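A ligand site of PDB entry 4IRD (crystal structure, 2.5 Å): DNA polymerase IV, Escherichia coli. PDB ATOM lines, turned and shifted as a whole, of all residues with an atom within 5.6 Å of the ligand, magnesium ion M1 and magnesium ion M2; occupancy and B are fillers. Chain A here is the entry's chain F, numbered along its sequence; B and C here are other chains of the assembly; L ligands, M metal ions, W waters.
OG of Ser 43 is in hydrogen-bond range of N2 of the ligand, 3.1 Å away.
The backbone NH (N) of Cys 12 sits at hydrogen-bond distance from an oxygen (O9) of the ligand (2.6 Å).
N4 of DC 14 of chain C is in hydrogen-bond range of a nitrogen (N3) of the ligand.
The side-chain hydroxyl of Thr 44 sits at hydrogen-bond distance from an oxygen (O5) of the ligand (2.8 Å).
O4 of DT 4 of chain B is in hydrogen-bond range of a nitrogen (N3) of the ligand, at 3.0 Å.
NH1 of Arg 50 lies within salt-bridge range of O6 of the ligand, at 3.3 Å.
The side-chain amino group of Lys 158 lies close to an oxygen (O3) of the ligand (3.99 Å).
O7 of the ligand is in hydrogen-bond range of N of Phe 14 of chain A.
The backbone NH (N) of Phe 13 sits at hydrogen-bond distance from an oxygen (O5) of the ligand (3.2 Å).
SG of Cys 12 lies within hydrogen-bond range of NH2 of Arg 50, at 3.2 Å.
O3' of DC 14 of chain C lies within hydrogen-bond range of OG of Ser 102, 2.8 Å away.
The backbone carbonyl oxygen (O) of Ser 43 lies within hydrogen-bond range of the side-chain hydroxyl (OG) of Ser 56, at 2.8 Å.
The backbone carbonyl oxygen (O) of Ala 45 sits at hydrogen-bond distance from the guanidinium group (NE) of Arg 50 (2.8 Å).
The side-chain carboxylate of Asp 11 lies within salt-bridge range of the side-chain amino group of Lys 158 (3.0 Å).
The guanidinium group (NH2) of Arg 50 is in hydrogen-bond range of the side-chain hydroxyl (OG1) of Thr 44 (3.2 Å).
SG of Cys 12 sits at hydrogen-bond distance from O of Ala 45, at 3.4 Å.
OG of Ser 102 is in hydrogen-bond range of OD2 of Asp 104 (3.2 Å).
A nitrogen (N1) of the ligand lies close to N1 of DG 5 of chain B (3.3 Å).
Residues that only touch the ligand: Asp 11 and Ser 56.
15 residues have an atom within 4 Å of the ligand: Asp 9, Met 10, Asp 11, Cys 12, Phe 13, Phe 14 of chain A, Ser 43, Thr 44, Arg 50, Ser 56, Asp 104, Lys 158, DT 4 of chain B, DG 5 of chain B and DC 14 of chain C.
Within 4 Å of magnesium ion M1: Asp 9, Met 10 and Asp 104.
The nearest printed residue that does not touch magnesium ion M1 is Cys 12 (4.4 Å).
Merely in contact with magnesium ion M2: DC 14 of chain C (3.4 Å).
Four residues have an atom within 4 Å of magnesium ion M2: Asp 9, Asp 104, Glu 105 and DC 14 of chain C.
Magnesium ion M1 is bound by OD1 of Asp 9 (2.0 Å), O3 of the ligand (2.1 Å), O1 of the ligand (2.2 Å), O of Met 10 (2.2 Å), O2 of the ligand (2.2 Å) and OD1 of Asp 104 (2.3 Å).
Magnesium ion M2 is bound by the side-chain carboxylate (OE1) of Glu 105 (2.1 Å) and an oxygen (O1) of the ligand (2.2 Å).
Magnesium ion M2 has two donor atoms within binding distance.
Slightly farther from magnesium ion M2 lies the side-chain carboxylate (OD2) of Asp 104 (2.7 Å).
Slightly farther from magnesium ion M2 lies water W3 (2.8 Å).
Water W3 lies within hydrogen-bond range of OD2 of Asp 9 (2.6 Å) and O4 of the ligand (3.2 Å).
Water W2 lies within hydrogen-bond range of O9 of the ligand (2.6 Å), OH of Tyr 47 (2.7 Å) and OD2 of Asp 11 (3.2 Å).
Water W1 lies within hydrogen-bond range of OG of Ser 43 (2.7 Å) and N2 of the ligand (2.7 Å).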
ATOM      1  N   ASP A   9     -26.215 -30.235   4.332  1.00  0.00           N
ATOM      2  CA  ASP A   9     -26.427 -29.643   5.660  1.00  0.00           C
ATOM      3  C   ASP A   9     -27.811 -29.989   6.113  1.00  0.00           C
ATOM      4  O   ASP A   9     -28.755 -29.669   5.440  1.00  0.00           O
ATOM      5  CB  ASP A   9     -26.277 -28.108   5.591  1.00  0.00           C
ATOM      6  CG  ASP A   9     -26.231 -27.469   6.955  1.00  0.00           C
ATOM      7  OD1 ASP A   9     -26.710 -28.096   7.933  1.00  0.00           O
ATOM      8  OD2 ASP A   9     -25.719 -26.336   7.029  1.00  0.00           O
ATOM      9  N   MET A  10     -27.931 -30.672   7.240  1.00  0.00           N
ATOM     10  CA  MET A  10     -29.235 -31.067   7.747  1.00  0.00           C
ATOM     11  C   MET A  10     -29.933 -29.863   8.313  1.00  0.00           C
ATOM     12  O   MET A  10     -29.282 -29.047   8.997  1.00  0.00           O
ATOM     13  CB  MET A  10     -29.093 -32.040   8.893  1.00  0.00           C
ATOM     14  CG  MET A  10     -28.320 -33.280   8.578  1.00  0.00           C
ATOM     15  SD  MET A  10     -29.239 -34.084   7.301  1.00  0.00           S
ATOM     16  CE  MET A  10     -30.563 -34.917   8.184  1.00  0.00           C
ATOM     17  N   ASP A  11     -31.254 -29.793   8.089  1.00  0.00           N
ATOM     18  CA  ASP A  11     -32.058 -28.677   8.573  1.00  0.00           C
ATOM     19  C   ASP A  11     -32.326 -28.717  10.079  1.00  0.00           C
ATOM     20  O   ASP A  11     -32.827 -29.729  10.585  1.00  0.00           O
ATOM     21  CB  ASP A  11     -33.360 -28.581   7.795  1.00  0.00           C
ATOM     22  CG  ASP A  11     -33.164 -28.351   6.319  1.00  0.00           C
ATOM     23  OD1 ASP A  11     -33.853 -29.017   5.503  1.00  0.00           O
ATOM     24  OD2 ASP A  11     -32.346 -27.470   5.934  1.00  0.00           O
ATOM     25  N   CYS A  12     -31.974 -27.642  10.796  1.00  0.00           N
ATOM     26  CA  CYS A  12     -32.362 -27.563  12.225  1.00  0.00           C
ATOM     27  C   CYS A  12     -32.033 -28.835  12.985  1.00  0.00           C
ATOM     28  O   CYS A  12     -32.945 -29.460  13.609  1.00  0.00           O
ATOM     29  CB  CYS A  12     -33.871 -27.417  12.304  1.00  0.00           C
ATOM     30  SG  CYS A  12     -34.311 -25.688  12.169  1.00  0.00           S
ATOM     31  N   PHE A  13     -30.762 -29.241  12.907  1.00  0.00           N
ATOM     32  CA  PHE A  13     -30.452 -30.648  13.039  1.00  0.00           C
ATOM     33  C   PHE A  13     -30.997 -31.202  14.361  1.00  0.00           C
ATOM     34  O   PHE A  13     -31.847 -32.092  14.331  1.00  0.00           O
ATOM     35  CB  PHE A  13     -28.961 -30.908  12.825  1.00  0.00           C
ATOM     36  CG  PHE A  13     -28.544 -32.348  13.044  1.00  0.00           C
ATOM     37  CD1 PHE A  13     -29.248 -33.386  12.488  1.00  0.00           C
ATOM     38  CD2 PHE A  13     -27.442 -32.652  13.831  1.00  0.00           C
ATOM     39  CE1 PHE A  13     -28.836 -34.692  12.702  1.00  0.00           C
ATOM     40  CE2 PHE A  13     -27.039 -33.954  14.047  1.00  0.00           C
ATOM     41  CZ  PHE A  13     -27.741 -34.983  13.480  1.00  0.00           C
ATOM     42  N   PHE A  14     -30.524 -30.690  15.487  1.00  0.00           N
ATOM     43  CA  PHE A  14     -30.934 -31.239  16.795  1.00  0.00           C
ATOM     44  C   PHE A  14     -32.432 -31.239  17.023  1.00  0.00           C
ATOM     45  O   PHE A  14     -33.005 -32.267  17.445  1.00  0.00           O
ATOM     46  CB  PHE A  14     -30.271 -30.508  17.945  1.00  0.00           C
ATOM     47  CG  PHE A  14     -28.826 -30.809  18.107  1.00  0.00           C
ATOM     48  CD1 PHE A  14     -28.131 -31.482  17.124  1.00  0.00           C
ATOM     49  CD2 PHE A  14     -28.141 -30.409  19.256  1.00  0.00           C
ATOM     50  CE1 PHE A  14     -26.759 -31.750  17.292  1.00  0.00           C
ATOM     51  CE2 PHE A  14     -26.799 -30.673  19.432  1.00  0.00           C
ATOM     52  CZ  PHE A  14     -26.100 -31.336  18.447  1.00  0.00           C
ATOM     53  N   ALA A  15     -33.052 -30.096  16.735  1.00  0.00           N
ATOM     54  CA  ALA A  15     -34.510 -29.978  16.844  1.00  0.00           C
ATOM     55  C   ALA A  15     -35.249 -30.928  15.910  1.00  0.00           C
ATOM     56  O   ALA A  15     -36.311 -31.430  16.267  1.00  0.00           O
ATOM     57  CB  ALA A  15     -34.940 -28.585  16.568  1.00  0.00           C
ATOM     58  N   VAL A  41     -26.888 -21.336  26.847  1.00  0.00           N
ATOM     59  CA  VAL A  41     -27.390 -20.761  25.605  1.00  0.00           C
ATOM     60  C   VAL A  41     -28.260 -21.737  24.840  1.00  0.00           C
ATOM     61  O   VAL A  41     -28.512 -22.859  25.278  1.00  0.00           O
ATOM     62  CB  VAL A  41     -26.247 -20.333  24.725  1.00  0.00           C
ATOM     63  CG1 VAL A  41     -25.349 -19.379  25.504  1.00  0.00           C
ATOM     64  CG2 VAL A  41     -25.476 -21.541  24.337  1.00  0.00           C
ATOM     65  N   ILE A  42     -28.763 -21.288  23.708  1.00  0.00           N
ATOM     66  CA  ILE A  42     -29.468 -22.181  22.804  1.00  0.00           C
ATOM     67  C   ILE A  42     -28.460 -22.793  21.821  1.00  0.00           C
ATOM     68  O   ILE A  42     -27.574 -22.120  21.284  1.00  0.00           O
ATOM     69  CB  ILE A  42     -30.520 -21.400  22.034  1.00  0.00           C
ATOM     70  CG1 ILE A  42     -31.549 -20.803  23.002  1.00  0.00           C
ATOM     71  CG2 ILE A  42     -31.060 -22.159  20.833  1.00  0.00           C
ATOM     72  CD1 ILE A  42     -32.656 -21.737  23.370  1.00  0.00           C
ATOM     73  N   SER A  43     -28.672 -24.092  21.678  1.00  0.00           N
ATOM     74  CA  SER A  43     -27.889 -24.918  20.803  1.00  0.00           C
ATOM     75  C   SER A  43     -28.504 -24.769  19.414  1.00  0.00           C
ATOM     76  O   SER A  43     -27.822 -24.416  18.459  1.00  0.00           O
ATOM     77  CB  SER A  43     -27.893 -26.388  21.266  1.00  0.00           C
ATOM     78  OG  SER A  43     -26.597 -26.798  21.647  1.00  0.00           O
ATOM     79  N   THR A  44     -29.802 -25.073  19.326  1.00  0.00           N
ATOM     80  CA  THR A  44     -30.533 -24.765  18.135  1.00  0.00           C
ATOM     81  C   THR A  44     -31.993 -24.604  18.438  1.00  0.00           C
ATOM     82  O   THR A  44     -32.406 -24.815  19.577  1.00  0.00           O
ATOM     83  CB  THR A  44     -30.352 -25.793  17.031  1.00  0.00           C
ATOM     84  OG1 THR A  44     -30.964 -25.247  15.860  1.00  0.00           O
ATOM     85  CG2 THR A  44     -31.036 -27.151  17.363  1.00  0.00           C
ATOM     86  N   ALA A  45     -32.762 -24.161  17.436  1.00  0.00           N
ATOM     87  CA  ALA A  45     -34.200 -24.075  17.603  1.00  0.00           C
ATOM     88  C   ALA A  45     -34.917 -24.468  16.348  1.00  0.00           C
ATOM     89  O   ALA A  45     -34.383 -24.298  15.284  1.00  0.00           O
ATOM     90  CB  ALA A  45     -34.623 -22.697  18.018  1.00  0.00           C
ATOM     91  N   TYR A  47     -38.220 -23.966  13.635  1.00  0.00           N
ATOM     92  CA  TYR A  47     -38.725 -22.821  12.915  1.00  0.00           C
ATOM     93  C   TYR A  47     -39.828 -22.060  13.667  1.00  0.00           C
ATOM     94  O   TYR A  47     -39.797 -20.819  13.787  1.00  0.00           O
ATOM     95  CB  TYR A  47     -39.122 -23.255  11.518  1.00  0.00           C
ATOM     96  CG  TYR A  47     -37.940 -23.187  10.572  1.00  0.00           C
ATOM     97  CD1 TYR A  47     -37.381 -24.336  10.028  1.00  0.00           C
ATOM     98  CD2 TYR A  47     -37.340 -21.952  10.278  1.00  0.00           C
ATOM     99  CE1 TYR A  47     -36.272 -24.262   9.194  1.00  0.00           C
ATOM    100  CE2 TYR A  47     -36.240 -21.851   9.444  1.00  0.00           C
ATOM    101  CZ  TYR A  47     -35.703 -23.001   8.907  1.00  0.00           C
ATOM    102  OH  TYR A  47     -34.614 -22.851   8.074  1.00  0.00           O
ATOM    103  N   ARG A  50     -37.646 -19.939  15.820  1.00  0.00           N
ATOM    104  CA  ARG A  50     -36.890 -18.943  15.084  1.00  0.00           C
ATOM    105  C   ARG A  50     -37.798 -17.751  14.723  1.00  0.00           C
ATOM    106  O   ARG A  50     -37.397 -16.577  14.813  1.00  0.00           O
ATOM    107  CB  ARG A  50     -36.278 -19.574  13.852  1.00  0.00           C
ATOM    108  CG  ARG A  50     -35.325 -20.703  14.178  1.00  0.00           C
ATOM    109  CD  ARG A  50     -34.620 -21.294  12.972  1.00  0.00           C
ATOM    110  NE  ARG A  50     -33.650 -22.308  13.381  1.00  0.00           N
ATOM    111  CZ  ARG A  50     -32.764 -22.920  12.605  1.00  0.00           C
ATOM    112  NH1 ARG A  50     -32.677 -22.670  11.300  1.00  0.00           N
ATOM    113  NH2 ARG A  50     -31.934 -23.795  13.147  1.00  0.00           N
ATOM    114  N   SER A  56     -29.157 -19.801  17.612  1.00  0.00           N
ATOM    115  CA  SER A  56     -28.075 -20.477  18.297  1.00  0.00           C
ATOM    116  C   SER A  56     -27.165 -19.443  18.915  1.00  0.00           C
ATOM    117  O   SER A  56     -26.968 -18.372  18.349  1.00  0.00           O
ATOM    118  CB  SER A  56     -27.264 -21.272  17.280  1.00  0.00           C
ATOM    119  OG  SER A  56     -28.011 -22.308  16.683  1.00  0.00           O
ATOM    120  N   ALA A  57     -26.584 -19.758  20.062  1.00  0.00           N
ATOM    121  CA  ALA A  57     -25.632 -18.846  20.726  1.00  0.00           C
ATOM    122  C   ALA A  57     -26.302 -17.838  21.667  1.00  0.00           C
ATOM    123  O   ALA A  57     -25.677 -17.305  22.577  1.00  0.00           O
ATOM    124  CB  ALA A  57     -24.732 -18.140  19.740  1.00  0.00           C
ATOM    125  N   SER A 102     -18.831 -31.507  10.781  1.00  0.00           N
ATOM    126  CA  SER A 102     -19.489 -31.534  12.046  1.00  0.00           C
ATOM    127  C   SER A 102     -20.447 -32.708  11.943  1.00  0.00           C
ATOM    128  O   SER A 102     -20.453 -33.395  10.943  1.00  0.00           O
ATOM    129  CB  SER A 102     -20.245 -30.253  12.251  1.00  0.00           C
ATOM    130  OG  SER A 102     -21.205 -30.081  11.228  1.00  0.00           O
ATOM    131  N   ASP A 104     -23.527 -32.723  11.243  1.00  0.00           N
ATOM    132  CA  ASP A 104     -24.640 -32.573  10.290  1.00  0.00           C
ATOM    133  C   ASP A 104     -24.249 -32.095   8.897  1.00  0.00           C
ATOM    134  O   ASP A 104     -25.116 -31.876   8.085  1.00  0.00           O
ATOM    135  CB  ASP A 104     -25.784 -31.705  10.842  1.00  0.00           C
ATOM    136  CG  ASP A 104     -25.506 -30.150  10.697  1.00  0.00           C
ATOM    137  OD1 ASP A 104     -26.500 -29.327  10.624  1.00  0.00           O
ATOM    138  OD2 ASP A 104     -24.306 -29.793  10.643  1.00  0.00           O
ATOM    139  N   GLU A 105     -22.956 -31.979   8.623  1.00  0.00           N
ATOM    140  CA  GLU A 105     -22.497 -31.303   7.410  1.00  0.00           C
ATOM    141  C   GLU A 105     -21.379 -32.088   6.820  1.00  0.00           C
ATOM    142  O   GLU A 105     -20.584 -32.602   7.592  1.00  0.00           O
ATOM    143  CB  GLU A 105     -21.894 -29.954   7.771  1.00  0.00           C
ATOM    144  CG  GLU A 105     -22.871 -28.843   7.958  1.00  0.00           C
ATOM    145  CD  GLU A 105     -22.177 -27.455   8.191  1.00  0.00           C
ATOM    146  OE1 GLU A 105     -22.907 -26.530   8.654  1.00  0.00           O
ATOM    147  OE2 GLU A 105     -20.937 -27.292   7.928  1.00  0.00           O
ATOM    148  N   ASP A 155     -27.383 -22.613   2.030  1.00  0.00           N
ATOM    149  CA  ASP A 155     -28.207 -21.880   2.971  1.00  0.00           C
ATOM    150  C   ASP A 155     -29.329 -21.200   2.203  1.00  0.00           C
ATOM    151  O   ASP A 155     -30.405 -20.962   2.735  1.00  0.00           O
ATOM    152  CB  ASP A 155     -27.394 -20.827   3.716  1.00  0.00           C
ATOM    153  CG  ASP A 155     -26.660 -21.413   4.909  1.00  0.00           C
ATOM    154  OD1 ASP A 155     -27.020 -22.524   5.395  1.00  0.00           O
ATOM    155  OD2 ASP A 155     -25.698 -20.736   5.365  1.00  0.00           O
ATOM    156  N   LYS A 158     -32.779 -23.073   2.119  1.00  0.00           N
ATOM    157  CA  LYS A 158     -33.159 -23.925   3.206  1.00  0.00           C
ATOM    158  C   LYS A 158     -34.441 -23.408   3.882  1.00  0.00           C
ATOM    159  O   LYS A 158     -34.692 -22.220   3.921  1.00  0.00           O
ATOM    160  CB  LYS A 158     -31.959 -24.140   4.129  1.00  0.00           C
ATOM    161  CG  LYS A 158     -31.962 -23.380   5.427  1.00  0.00           C
ATOM    162  CD  LYS A 158     -30.571 -23.460   6.067  1.00  0.00           C
ATOM    163  CE  LYS A 158     -30.254 -24.812   6.700  1.00  0.00           C
ATOM    164  NZ  LYS A 158     -29.809 -25.943   5.824  1.00  0.00           N
ATOM    165  P    DT B   4     -21.426 -18.911  28.117  1.00  0.00           P
ATOM    166  OP1  DT B   4     -21.485 -19.015  29.583  1.00  0.00           O
ATOM    167  OP2  DT B   4     -20.139 -18.546  27.450  1.00  0.00           O
ATOM    168  O5'  DT B   4     -22.057 -20.279  27.629  1.00  0.00           O
ATOM    169  C5'  DT B   4     -23.065 -20.879  28.421  1.00  0.00           C
ATOM    170  C4'  DT B   4     -22.959 -22.378  28.248  1.00  0.00           C
ATOM    171  O4'  DT B   4     -23.358 -22.725  26.909  1.00  0.00           O
ATOM    172  C3'  DT B   4     -21.576 -22.989  28.440  1.00  0.00           C
ATOM    173  O3'  DT B   4     -21.766 -24.303  28.953  1.00  0.00           O
ATOM    174  C2'  DT B   4     -21.014 -23.073  27.040  1.00  0.00           C
ATOM    175  C1'  DT B   4     -22.264 -23.256  26.180  1.00  0.00           C
ATOM    176  N1   DT B   4     -22.242 -22.601  24.883  1.00  0.00           N
ATOM    177  C2   DT B   4     -22.790 -23.279  23.825  1.00  0.00           C
ATOM    178  O2   DT B   4     -23.272 -24.386  23.928  1.00  0.00           O
ATOM    179  N3   DT B   4     -22.739 -22.610  22.623  1.00  0.00           N
ATOM    180  C4   DT B   4     -22.264 -21.318  22.410  1.00  0.00           C
ATOM    181  O4   DT B   4     -22.308 -20.838  21.283  1.00  0.00           O
ATOM    182  C5   DT B   4     -21.742 -20.655  23.578  1.00  0.00           C
ATOM    183  C7   DT B   4     -21.193 -19.273  23.445  1.00  0.00           C
ATOM    184  C6   DT B   4     -21.757 -21.324  24.740  1.00  0.00           C
ATOM    185  P    DG B   5     -20.540 -25.089  29.555  1.00  0.00           P
ATOM    186  OP1  DG B   5     -21.030 -25.820  30.748  1.00  0.00           O
ATOM    187  OP2  DG B   5     -19.377 -24.163  29.638  1.00  0.00           O
ATOM    188  O5'  DG B   5     -20.203 -26.109  28.380  1.00  0.00           O
ATOM    189  C5'  DG B   5     -21.159 -27.085  27.927  1.00  0.00           C
ATOM    190  C4'  DG B   5     -20.516 -27.877  26.818  1.00  0.00           C
ATOM    191  O4'  DG B   5     -20.614 -27.139  25.568  1.00  0.00           O
ATOM    192  C3'  DG B   5     -19.027 -28.148  27.008  1.00  0.00           C
ATOM    193  O3'  DG B   5     -18.799 -29.366  26.304  1.00  0.00           O
ATOM    194  C2'  DG B   5     -18.388 -27.005  26.244  1.00  0.00           C
ATOM    195  C1'  DG B   5     -19.318 -26.943  25.042  1.00  0.00           C
ATOM    196  N9   DG B   5     -19.288 -25.684  24.293  1.00  0.00           N
ATOM    197  C8   DG B   5     -18.768 -24.497  24.725  1.00  0.00           C
ATOM    198  N7   DG B   5     -18.814 -23.560  23.824  1.00  0.00           N
ATOM    199  C5   DG B   5     -19.355 -24.173  22.710  1.00  0.00           C
ATOM    200  C6   DG B   5     -19.638 -23.659  21.415  1.00  0.00           C
ATOM    201  O6   DG B   5     -19.448 -22.522  20.972  1.00  0.00           O
ATOM    202  N1   DG B   5     -20.204 -24.634  20.593  1.00  0.00           N
ATOM    203  C2   DG B   5     -20.433 -25.932  20.961  1.00  0.00           C
ATOM    204  N2   DG B   5     -20.962 -26.722  20.017  1.00  0.00           N
ATOM    205  N3   DG B   5     -20.220 -26.408  22.168  1.00  0.00           N
ATOM    206  C4   DG B   5     -19.662 -25.496  22.985  1.00  0.00           C
ATOM    207  P    DC C  14     -20.282 -23.360  10.366  1.00  0.00           P
ATOM    208  OP1  DC C  14     -20.297 -24.260   9.182  1.00  0.00           O
ATOM    209  OP2  DC C  14     -21.203 -22.189  10.526  1.00  0.00           O
ATOM    210  O5'  DC C  14     -20.457 -24.420  11.545  1.00  0.00           O
ATOM    211  C5'  DC C  14     -19.975 -25.751  11.381  1.00  0.00           C
ATOM    212  C4'  DC C  14     -20.571 -26.607  12.473  1.00  0.00           C
ATOM    213  O4'  DC C  14     -20.191 -25.999  13.731  1.00  0.00           O
ATOM    214  C3'  DC C  14     -22.093 -26.666  12.472  1.00  0.00           C
ATOM    215  O3'  DC C  14     -22.499 -28.033  12.609  1.00  0.00           O
ATOM    216  C2'  DC C  14     -22.496 -25.852  13.694  1.00  0.00           C
ATOM    217  C1'  DC C  14     -21.294 -25.960  14.601  1.00  0.00           C
ATOM    218  N1   DC C  14     -21.081 -24.817  15.505  1.00  0.00           N
ATOM    219  C2   DC C  14     -20.860 -25.085  16.856  1.00  0.00           C
ATOM    220  O2   DC C  14     -20.896 -26.254  17.251  1.00  0.00           O
ATOM    221  N3   DC C  14     -20.615 -24.054  17.695  1.00  0.00           N
ATOM    222  C4   DC C  14     -20.571 -22.811  17.233  1.00  0.00           C
ATOM    223  N4   DC C  14     -20.329 -21.829  18.106  1.00  0.00           N
ATOM    224  C5   DC C  14     -20.781 -22.508  15.857  1.00  0.00           C
ATOM    225  C6   DC C  14     -21.000 -23.537  15.031  1.00  0.00           C
HETATM  226  N1  LIG L   1     -23.405 -23.972  20.274  1.00  0.00           N
HETATM  227  C1  LIG L   1     -23.726 -25.292  20.532  1.00  0.00           C
HETATM  228  N2  LIG L   1     -24.283 -26.094  19.638  1.00  0.00           N
HETATM  229  C2  LIG L   1     -24.542 -25.663  18.372  1.00  0.00           C
HETATM  230  C3  LIG L   1     -24.223 -24.280  18.028  1.00  0.00           C
HETATM  231  C4  LIG L   1     -23.643 -23.445  19.050  1.00  0.00           C
HETATM  232  N3  LIG L   1     -23.361 -22.168  18.763  1.00  0.00           N
HETATM  233  N4  LIG L   1     -24.570 -24.076  16.754  1.00  0.00           N
HETATM  234  C5  LIG L   1     -25.060 -25.259  16.294  1.00  0.00           C
HETATM  235  N5  LIG L   1     -25.079 -26.200  17.263  1.00  0.00           N
HETATM  236  P1  LIG L   1     -26.113 -25.800  12.208  1.00  0.00           P
HETATM  237  P2  LIG L   1     -29.001 -26.153  12.343  1.00  0.00           P
HETATM  238  P3  LIG L   1     -29.980 -24.930  10.108  1.00  0.00           P
HETATM  239  C6  LIG L   1     -25.535 -27.606  17.022  1.00  0.00           C
HETATM  240  O1  LIG L   1     -26.316 -26.538  10.900  1.00  0.00           O
HETATM  241  O2  LIG L   1     -28.708 -27.428  11.594  1.00  0.00           O
HETATM  242  O3  LIG L   1     -28.811 -25.832   9.686  1.00  0.00           O
HETATM  243  C7  LIG L   1     -27.037 -27.672  17.027  1.00  0.00           C
HETATM  244  O4  LIG L   1     -25.348 -24.408  12.247  1.00  0.00           O
HETATM  245  O5  LIG L   1     -29.561 -26.347  13.735  1.00  0.00           O
HETATM  246  O6  LIG L   1     -29.872 -23.486   9.702  1.00  0.00           O
HETATM  247  C8  LIG L   1     -27.373 -27.592  15.569  1.00  0.00           C
HETATM  248  O7  LIG L   1     -28.573 -28.305  15.331  1.00  0.00           O
HETATM  249  N6  LIG L   1     -27.617 -25.359  12.623  1.00  0.00           N
HETATM  250  O8  LIG L   1     -29.947 -25.081  11.677  1.00  0.00           O
HETATM  251  O9  LIG L   1     -31.321 -25.423   9.688  1.00  0.00           O
HETATM  252  C9  LIG L   1     -26.217 -28.354  14.948  1.00  0.00           C
HETATM  253  O10 LIG L   1     -25.095 -27.979  15.687  1.00  0.00           O
HETATM  254  C10 LIG L   1     -25.965 -28.050  13.464  1.00  0.00           C
HETATM  255  O11 LIG L   1     -25.431 -26.755  13.298  1.00  0.00           O
HETATM  256 MG    MG M   1     -27.724 -27.602   9.615  1.00  0.00          MG
HETATM  257 MG    MG M   2     -24.396 -27.143   9.983  1.00  0.00          MG
HETATM  258  O   HOH W   1     -24.572 -28.475  20.940  1.00  0.00           O
HETATM  259  O   HOH W   2     -33.361 -25.255   8.022  1.00  0.00           O
HETATM  260  O   HOH W   3     -25.791 -24.818   9.146  1.00  0.00           O
